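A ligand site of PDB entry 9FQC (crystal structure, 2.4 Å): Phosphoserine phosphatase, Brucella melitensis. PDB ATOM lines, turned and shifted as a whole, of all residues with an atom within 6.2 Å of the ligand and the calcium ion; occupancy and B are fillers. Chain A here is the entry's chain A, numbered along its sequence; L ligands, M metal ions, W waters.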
ATOM      1  N   ASP A  98      15.009   0.370 -10.276  1.00  0.00           N
ATOM      2  CA  ASP A  98      14.898   1.389  -9.246  1.00  0.00           C
ATOM      3  C   ASP A  98      15.854   2.543  -9.517  1.00  0.00           C
ATOM      4  O   ASP A  98      16.905   2.365 -10.138  1.00  0.00           O
ATOM      5  CB  ASP A  98      15.224   0.727  -7.912  1.00  0.00           C
ATOM      6  CG  ASP A  98      15.225   1.678  -6.780  1.00  0.00           C
ATOM      7  OD1 ASP A  98      14.180   2.324  -6.534  1.00  0.00           O
ATOM      8  OD2 ASP A  98      16.270   1.780  -6.117  1.00  0.00           O
ATOM      9  N   MET A  99      15.500   3.752  -9.049  1.00  0.00           N
ATOM     10  CA  MET A  99      16.440   4.860  -9.252  1.00  0.00           C
ATOM     11  C   MET A  99      17.315   5.173  -8.033  1.00  0.00           C
ATOM     12  O   MET A  99      18.541   5.080  -8.129  1.00  0.00           O
ATOM     13  CB  MET A  99      15.739   6.164  -9.665  1.00  0.00           C
ATOM     14  CG  MET A  99      16.729   7.342  -9.641  1.00  0.00           C
ATOM     15  SD  MET A  99      16.148   8.886 -10.364  1.00  0.00           S
ATOM     16  CE  MET A  99      15.135   9.472  -8.971  1.00  0.00           C
ATOM     17  N   ASP A 100      16.714   5.576  -6.911  1.00  0.00           N
ATOM     18  CA  ASP A 100      17.473   6.085  -5.774  1.00  0.00           C
ATOM     19  C   ASP A 100      18.313   4.991  -5.126  1.00  0.00           C
ATOM     20  O   ASP A 100      17.795   3.913  -4.785  1.00  0.00           O
ATOM     21  CB  ASP A 100      16.543   6.713  -4.721  1.00  0.00           C
ATOM     22  CG  ASP A 100      16.178   8.159  -5.036  1.00  0.00           C
ATOM     23  OD1 ASP A 100      16.575   8.721  -6.081  1.00  0.00           O
ATOM     24  OD2 ASP A 100      15.480   8.770  -4.215  1.00  0.00           O
ATOM     25  N   SER A 101      19.598   5.282  -4.932  1.00  0.00           N
ATOM     26  CA  SER A 101      20.601   4.385  -4.373  1.00  0.00           C
ATOM     27  C   SER A 101      20.879   3.185  -5.255  1.00  0.00           C
ATOM     28  O   SER A 101      21.637   2.305  -4.844  1.00  0.00           O
ATOM     29  CB  SER A 101      20.230   3.914  -2.958  1.00  0.00           C
ATOM     30  OG  SER A 101      20.229   5.000  -2.065  1.00  0.00           O
ATOM     31  N   THR A 102      20.291   3.114  -6.441  1.00  0.00           N
ATOM     32  CA  THR A 102      20.549   2.047  -7.401  1.00  0.00           C
ATOM     33  C   THR A 102      21.240   2.583  -8.646  1.00  0.00           C
ATOM     34  O   THR A 102      22.421   2.292  -8.864  1.00  0.00           O
ATOM     35  CB  THR A 102      19.241   1.320  -7.744  1.00  0.00           C
ATOM     36  OG1 THR A 102      18.710   0.678  -6.570  1.00  0.00           O
ATOM     37  CG2 THR A 102      19.439   0.250  -8.812  1.00  0.00           C
ATOM     38  N   GLU A 107      19.782   9.625  -2.354  1.00  0.00           N
ATOM     39  CA  GLU A 107      18.333   9.688  -2.195  1.00  0.00           C
ATOM     40  C   GLU A 107      17.916  11.120  -2.488  1.00  0.00           C
ATOM     41  O   GLU A 107      18.231  12.026  -1.711  1.00  0.00           O
ATOM     42  CB  GLU A 107      17.911   9.265  -0.791  1.00  0.00           C
ATOM     43  CG  GLU A 107      18.375   7.882  -0.403  1.00  0.00           C
ATOM     44  CD  GLU A 107      17.440   6.807  -0.916  1.00  0.00           C
ATOM     45  OE1 GLU A 107      16.311   7.136  -1.324  1.00  0.00           O
ATOM     46  OE2 GLU A 107      17.846   5.628  -0.945  1.00  0.00           O
ATOM     47  N   CYS A 108      17.216  11.340  -3.602  1.00  0.00           N
ATOM     48  CA  CYS A 108      16.864  12.708  -3.964  1.00  0.00           C
ATOM     49  C   CYS A 108      16.068  13.386  -2.864  1.00  0.00           C
ATOM     50  O   CYS A 108      16.252  14.582  -2.623  1.00  0.00           O
ATOM     51  CB  CYS A 108      16.072  12.724  -5.268  1.00  0.00           C
ATOM     52  SG  CYS A 108      16.924  11.950  -6.629  1.00  0.00           S
ATOM     53  N   ILE A 109      15.220  12.633  -2.169  1.00  0.00           N
ATOM     54  CA  ILE A 109      14.413  13.221  -1.103  1.00  0.00           C
ATOM     55  C   ILE A 109      15.293  13.700   0.055  1.00  0.00           C
ATOM     56  O   ILE A 109      15.042  14.760   0.635  1.00  0.00           O
ATOM     57  CB  ILE A 109      13.340  12.213  -0.645  1.00  0.00           C
ATOM     58  CG1 ILE A 109      12.548  12.755   0.538  1.00  0.00           C
ATOM     59  CG2 ILE A 109      13.967  10.881  -0.264  1.00  0.00           C
ATOM     60  CD1 ILE A 109      11.431  13.691   0.142  1.00  0.00           C
ATOM     61  N   THR A 126      13.737   7.918   5.695  1.00  0.00           N
ATOM     62  CA  THR A 126      14.031   7.194   4.465  1.00  0.00           C
ATOM     63  C   THR A 126      14.638   5.825   4.752  1.00  0.00           C
ATOM     64  O   THR A 126      14.244   4.822   4.146  1.00  0.00           O
ATOM     65  CB  THR A 126      14.985   8.026   3.605  1.00  0.00           C
ATOM     66  OG1 THR A 126      14.365   9.272   3.311  1.00  0.00           O
ATOM     67  CG2 THR A 126      15.315   7.321   2.300  1.00  0.00           C
ATOM     68  N   ALA A 129      11.955   3.548   5.776  1.00  0.00           N
ATOM     69  CA  ALA A 129      11.070   3.187   4.674  1.00  0.00           C
ATOM     70  C   ALA A 129      11.724   2.178   3.743  1.00  0.00           C
ATOM     71  O   ALA A 129      11.095   1.191   3.333  1.00  0.00           O
ATOM     72  CB  ALA A 129      10.654   4.444   3.892  1.00  0.00           C
ATOM     73  N   MET A 130      12.988   2.406   3.383  1.00  0.00           N
ATOM     74  CA  MET A 130      13.651   1.458   2.491  1.00  0.00           C
ATOM     75  C   MET A 130      13.968   0.138   3.178  1.00  0.00           C
ATOM     76  O   MET A 130      14.138  -0.876   2.493  1.00  0.00           O
ATOM     77  CB  MET A 130      14.902   2.099   1.903  1.00  0.00           C
ATOM     78  CG  MET A 130      14.603   3.359   1.065  1.00  0.00           C
ATOM     79  SD  MET A 130      13.695   3.094  -0.495  1.00  0.00           S
ATOM     80  CE  MET A 130      11.962   3.151  -0.001  1.00  0.00           C
ATOM     81  N   PHE A 136       5.561   2.739   2.399  1.00  0.00           N
ATOM     82  CA  PHE A 136       6.178   3.768   1.573  1.00  0.00           C
ATOM     83  C   PHE A 136       5.346   5.046   1.530  1.00  0.00           C
ATOM     84  O   PHE A 136       5.895   6.151   1.641  1.00  0.00           O
ATOM     85  CB  PHE A 136       6.433   3.266   0.160  1.00  0.00           C
ATOM     86  CG  PHE A 136       7.067   4.299  -0.714  1.00  0.00           C
ATOM     87  CD1 PHE A 136       8.429   4.542  -0.621  1.00  0.00           C
ATOM     88  CD2 PHE A 136       6.292   5.063  -1.588  1.00  0.00           C
ATOM     89  CE1 PHE A 136       9.039   5.510  -1.406  1.00  0.00           C
ATOM     90  CE2 PHE A 136       6.899   6.032  -2.386  1.00  0.00           C
ATOM     91  CZ  PHE A 136       8.278   6.259  -2.293  1.00  0.00           C
ATOM     92  N   LEU A 140       6.486   8.799   2.517  1.00  0.00           N
ATOM     93  CA  LEU A 140       6.717   9.828   1.510  1.00  0.00           C
ATOM     94  C   LEU A 140       6.014  11.141   1.853  1.00  0.00           C
ATOM     95  O   LEU A 140       6.618  12.214   1.760  1.00  0.00           O
ATOM     96  CB  LEU A 140       6.271   9.349   0.128  1.00  0.00           C
ATOM     97  CG  LEU A 140       6.618  10.231  -1.067  1.00  0.00           C
ATOM     98  CD1 LEU A 140       8.138  10.440  -1.172  1.00  0.00           C
ATOM     99  CD2 LEU A 140       6.074   9.659  -2.369  1.00  0.00           C
ATOM    100  N   ARG A 143       7.815  12.967   4.646  1.00  0.00           N
ATOM    101  CA  ARG A 143       9.068  13.599   4.242  1.00  0.00           C
ATOM    102  C   ARG A 143       8.824  14.808   3.338  1.00  0.00           C
ATOM    103  O   ARG A 143       9.446  15.857   3.519  1.00  0.00           O
ATOM    104  CB  ARG A 143       9.960  12.587   3.543  1.00  0.00           C
ATOM    105  CG  ARG A 143      10.574  11.614   4.521  1.00  0.00           C
ATOM    106  CD  ARG A 143      11.339  10.529   3.795  1.00  0.00           C
ATOM    107  NE  ARG A 143      10.432   9.610   3.110  1.00  0.00           N
ATOM    108  CZ  ARG A 143      10.822   8.742   2.180  1.00  0.00           C
ATOM    109  NH1 ARG A 143      12.089   8.653   1.798  1.00  0.00           N
ATOM    110  NH2 ARG A 143       9.918   7.951   1.609  1.00  0.00           N
ATOM    111  N   VAL A 186      12.046   3.171 -12.911  1.00  0.00           N
ATOM    112  CA  VAL A 186      10.752   3.199 -12.238  1.00  0.00           C
ATOM    113  C   VAL A 186      11.009   3.447 -10.739  1.00  0.00           C
ATOM    114  O   VAL A 186      11.603   2.604 -10.055  1.00  0.00           O
ATOM    115  CB  VAL A 186       9.979   1.893 -12.471  1.00  0.00           C
ATOM    116  CG1 VAL A 186       8.708   1.863 -11.640  1.00  0.00           C
ATOM    117  CG2 VAL A 186       9.686   1.710 -13.954  1.00  0.00           C
ATOM    118  N   SER A 187      10.515   4.577 -10.237  1.00  0.00           N
ATOM    119  CA  SER A 187      11.000   5.136  -8.985  1.00  0.00           C
ATOM    120  C   SER A 187       9.831   5.641  -8.130  1.00  0.00           C
ATOM    121  O   SER A 187       8.816   6.121  -8.655  1.00  0.00           O
ATOM    122  CB  SER A 187      12.004   6.263  -9.272  1.00  0.00           C
ATOM    123  OG  SER A 187      12.271   7.052  -8.136  1.00  0.00           O
ATOM    124  N   GLY A 188       9.997   5.517  -6.814  1.00  0.00           N
ATOM    125  CA  GLY A 188       9.131   6.186  -5.872  1.00  0.00           C
ATOM    126  C   GLY A 188       9.495   7.638  -5.632  1.00  0.00           C
ATOM    127  O   GLY A 188       8.781   8.337  -4.924  1.00  0.00           O
ATOM    128  N   GLY A 189      10.614   8.080  -6.227  1.00  0.00           N
ATOM    129  CA  GLY A 189      11.003   9.490  -6.227  1.00  0.00           C
ATOM    130  C   GLY A 189      10.212  10.311  -7.210  1.00  0.00           C
ATOM    131  O   GLY A 189       9.038  10.035  -7.487  1.00  0.00           O
ATOM    132  N   PHE A 190      10.853  11.345  -7.776  1.00  0.00           N
ATOM    133  CA  PHE A 190      10.102  12.410  -8.431  1.00  0.00           C
ATOM    134  C   PHE A 190      10.440  12.564  -9.908  1.00  0.00           C
ATOM    135  O   PHE A 190      11.616  12.484 -10.314  1.00  0.00           O
ATOM    136  CB  PHE A 190      10.323  13.725  -7.695  1.00  0.00           C
ATOM    137  CG  PHE A 190      10.140  13.583  -6.210  1.00  0.00           C
ATOM    138  CD1 PHE A 190       8.912  13.207  -5.681  1.00  0.00           C
ATOM    139  CD2 PHE A 190      11.212  13.752  -5.343  1.00  0.00           C
ATOM    140  CE1 PHE A 190       8.737  13.039  -4.312  1.00  0.00           C
ATOM    141  CE2 PHE A 190      11.056  13.599  -3.979  1.00  0.00           C
ATOM    142  CZ  PHE A 190       9.803  13.232  -3.464  1.00  0.00           C
ATOM    143  N   LYS A 232       5.066  -0.431  -8.692  1.00  0.00           N
ATOM    144  CA  LYS A 232       6.172  -0.935  -9.499  1.00  0.00           C
ATOM    145  C   LYS A 232       5.812  -2.277 -10.130  1.00  0.00           C
ATOM    146  O   LYS A 232       6.178  -2.539 -11.282  1.00  0.00           O
ATOM    147  CB  LYS A 232       7.457  -1.048  -8.667  1.00  0.00           C
ATOM    148  CG  LYS A 232       7.942   0.284  -8.074  1.00  0.00           C
ATOM    149  CD  LYS A 232       9.447   0.292  -7.777  1.00  0.00           C
ATOM    150  CE  LYS A 232       9.871   1.592  -7.072  1.00  0.00           C
ATOM    151  NZ  LYS A 232      11.338   1.934  -7.261  1.00  0.00           N
ATOM    152  N   GLY A 254      16.811  -3.529  -7.550  1.00  0.00           N
ATOM    153  CA  GLY A 254      16.536  -2.498  -6.581  1.00  0.00           C
ATOM    154  C   GLY A 254      17.296  -2.768  -5.304  1.00  0.00           C
ATOM    155  O   GLY A 254      17.939  -3.813  -5.148  1.00  0.00           O
ATOM    156  N   ASP A 255      17.201  -1.808  -4.380  1.00  0.00           N
ATOM    157  CA  ASP A 255      17.837  -1.879  -3.064  1.00  0.00           C
ATOM    158  C   ASP A 255      16.865  -1.836  -1.894  1.00  0.00           C
ATOM    159  O   ASP A 255      17.289  -2.080  -0.767  1.00  0.00           O
ATOM    160  CB  ASP A 255      18.823  -0.719  -2.892  1.00  0.00           C
ATOM    161  CG  ASP A 255      18.108   0.618  -2.706  1.00  0.00           C
ATOM    162  OD1 ASP A 255      17.288   0.965  -3.574  1.00  0.00           O
ATOM    163  OD2 ASP A 255      18.325   1.317  -1.704  1.00  0.00           O
ATOM    164  N   GLY A 256      15.596  -1.490  -2.125  1.00  0.00           N
ATOM    165  CA  GLY A 256      14.700  -1.126  -1.053  1.00  0.00           C
ATOM    166  C   GLY A 256      13.449  -2.005  -0.989  1.00  0.00           C
ATOM    167  O   GLY A 256      13.119  -2.739  -1.917  1.00  0.00           O
ATOM    168  N   ASN A 258      10.364  -1.201  -1.201  1.00  0.00           N
ATOM    169  CA  ASN A 258       9.420  -0.889  -2.271  1.00  0.00           C
ATOM    170  C   ASN A 258       9.794  -1.524  -3.613  1.00  0.00           C
ATOM    171  O   ASN A 258       8.998  -1.407  -4.551  1.00  0.00           O
ATOM    172  CB  ASN A 258       9.291   0.639  -2.427  1.00  0.00           C
ATOM    173  CG  ASN A 258      10.609   1.281  -2.834  1.00  0.00           C
ATOM    174  OD1 ASN A 258      11.672   0.794  -2.442  1.00  0.00           O
ATOM    175  ND2 ASN A 258      10.553   2.387  -3.580  1.00  0.00           N
ATOM    176  N   ASP A 259      10.947  -2.163  -3.749  1.00  0.00           N
ATOM    177  CA  ASP A 259      11.281  -2.868  -4.974  1.00  0.00           C
ATOM    178  C   ASP A 259      10.981  -4.359  -4.903  1.00  0.00           C
ATOM    179  O   ASP A 259      11.137  -5.056  -5.912  1.00  0.00           O
ATOM    180  CB  ASP A 259      12.755  -2.700  -5.343  1.00  0.00           C
ATOM    181  CG  ASP A 259      13.158  -1.244  -5.469  1.00  0.00           C
ATOM    182  OD1 ASP A 259      12.461  -0.536  -6.215  1.00  0.00           O
ATOM    183  OD2 ASP A 259      14.178  -0.839  -4.839  1.00  0.00           O
ATOM    184  N   LYS A 275      19.284  -3.130   1.446  1.00  0.00           N
ATOM    185  CA  LYS A 275      19.050  -3.003   2.880  1.00  0.00           C
ATOM    186  C   LYS A 275      19.027  -4.379   3.566  1.00  0.00           C
ATOM    187  O   LYS A 275      18.658  -5.391   2.951  1.00  0.00           O
ATOM    188  CB  LYS A 275      17.757  -2.222   3.114  1.00  0.00           C
ATOM    189  CG  LYS A 275      17.643  -0.971   2.257  1.00  0.00           C
ATOM    190  CD  LYS A 275      18.775   0.025   2.498  1.00  0.00           C
ATOM    191  CE  LYS A 275      18.535   1.361   1.789  1.00  0.00           C
ATOM    192  NZ  LYS A 275      19.570   1.658   0.747  1.00  0.00           N
HETATM  193  N1  LIG L   1      14.141   5.887  -2.242  1.00  0.00           N
HETATM  194  C1  LIG L   1      13.107   6.914  -2.477  1.00  0.00           C
HETATM  195  C2  LIG L   1      12.132   6.425  -3.578  1.00  0.00           C
HETATM  196  O1  LIG L   1      12.847   6.458  -4.755  1.00  0.00           O
HETATM  197  C3  LIG L   1      12.340   7.227  -1.195  1.00  0.00           C
HETATM  198  O2  LIG L   1      12.622   6.682  -0.120  1.00  0.00           O
HETATM  199  O3  LIG L   1      11.391   8.079  -1.323  1.00  0.00           O
HETATM  200  P1  LIG L   1      13.367   4.895  -5.451  1.00  0.00           P
HETATM  201  O4  LIG L   1      13.936   5.354  -6.799  1.00  0.00           O
HETATM  202  O5  LIG L   1      14.322   4.358  -4.403  1.00  0.00           O
HETATM  203  O6  LIG L   1      12.019   4.142  -5.503  1.00  0.00           O
HETATM  204 CA    CA M   1      15.901   2.740  -4.039  1.00  0.00          CA
HETATM  205  O   HOH W   1      16.502   3.418  -1.902  1.00  0.00           O
HETATM  206  O   HOH W   2      14.130   1.312  -3.492  1.00  0.00           O
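OD2 of Asp 100 is in hydrogen-bond range of N of Cys 108, 3.2 Å away. The backbone NH (N) of Asp 255 sits at hydrogen-bond distance from the side-chain carboxylate (OD2) of Asp 259 (3.2 Å). The side-chain sulfur (SD) of Met 130 lies close to the side-chain amide oxygen (OD1) of Asn 258 (3.6 Å). OE2 of Glu 107 lies within hydrogen-bond range of OG of Ser 101 (2.7 Å). The side-chain carboxylate (OD2) of Asp 98 sits close to the side-chain hydroxyl (OG1) of Thr 102 (2.7 Å). The side-chain hydroxyl (OG1) of Thr 102 sits close to the side-chain carboxylate (OD1) of Asp 255 (3.3 Å). NZ of Lys 232 lies within salt-bridge range of OD1 of Asp 259, 2.9 Å away. OG of Ser 187 sits at hydrogen-bond distance from N of Gly 189 (2.7 Å).
The calcium ion is bound by an oxygen (O5) of the ligand (2.3 Å), the side-chain carboxylate of Asp 255 (2.3 Å), the side-chain carboxylate of Asp 98 (2.3 Å), water W1 (2.3 Å), water W2 (2.3 Å) and the backbone carbonyl oxygen of Asp 100 (2.3 Å). The calcium ion has six donor atoms within binding distance. Slightly farther from the calcium ion lies the side-chain carboxylate (OD1) of Asp 98 (3.1 Å).
Of the 26 residues printed, 3 come within 4 Å of the calcium ion. The nearest printed residue that does not touch the calcium ion is Asp 259 (4.1 Å).
The side-chain amide nitrogen (ND2) of Asn 258 lies within hydrogen-bond range of an oxygen (O6) of the ligand, at 3.0 Å. The guanidinium group of Arg 143 lies within salt-bridge range of an oxygen (O2) of the ligand, at 2.8 Å. The side-chain carboxylate of Asp 100 is in salt-bridge range of a nitrogen (N1) of the ligand, at 3.7 Å. A nitrogen (N1) of the ligand is in hydrogen-bond range of the side-chain sulfur of Met 130. N of Gly 189 lies within hydrogen-bond range of O1 of the ligand, 3.1 Å away. O6 of the ligand lies within salt-bridge range of NZ of Lys 232, at 2.9 Å. OE1 of Glu 107 is in salt-bridge range of N1 of the ligand, 2.7 Å away. OG of Ser 187 lies within hydrogen-bond range of O4 of the ligand, at 2.7 Å. The backbone NH of Met 99 lies within hydrogen-bond range of an oxygen (O4) of the ligand (3.2 Å). The backbone NH (N) of Gly 188 lies within hydrogen-bond range of an oxygen (O6) of the ligand, at 2.8 Å. N of Asp 100 lies within hydrogen-bond range of O4 of the ligand, at 2.8 Å.
Merely in contact with the ligand: Ile 109, Thr 126 and Phe 136. The nearest printed residue that does not touch the ligand is Leu 140 (4.02 Å).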
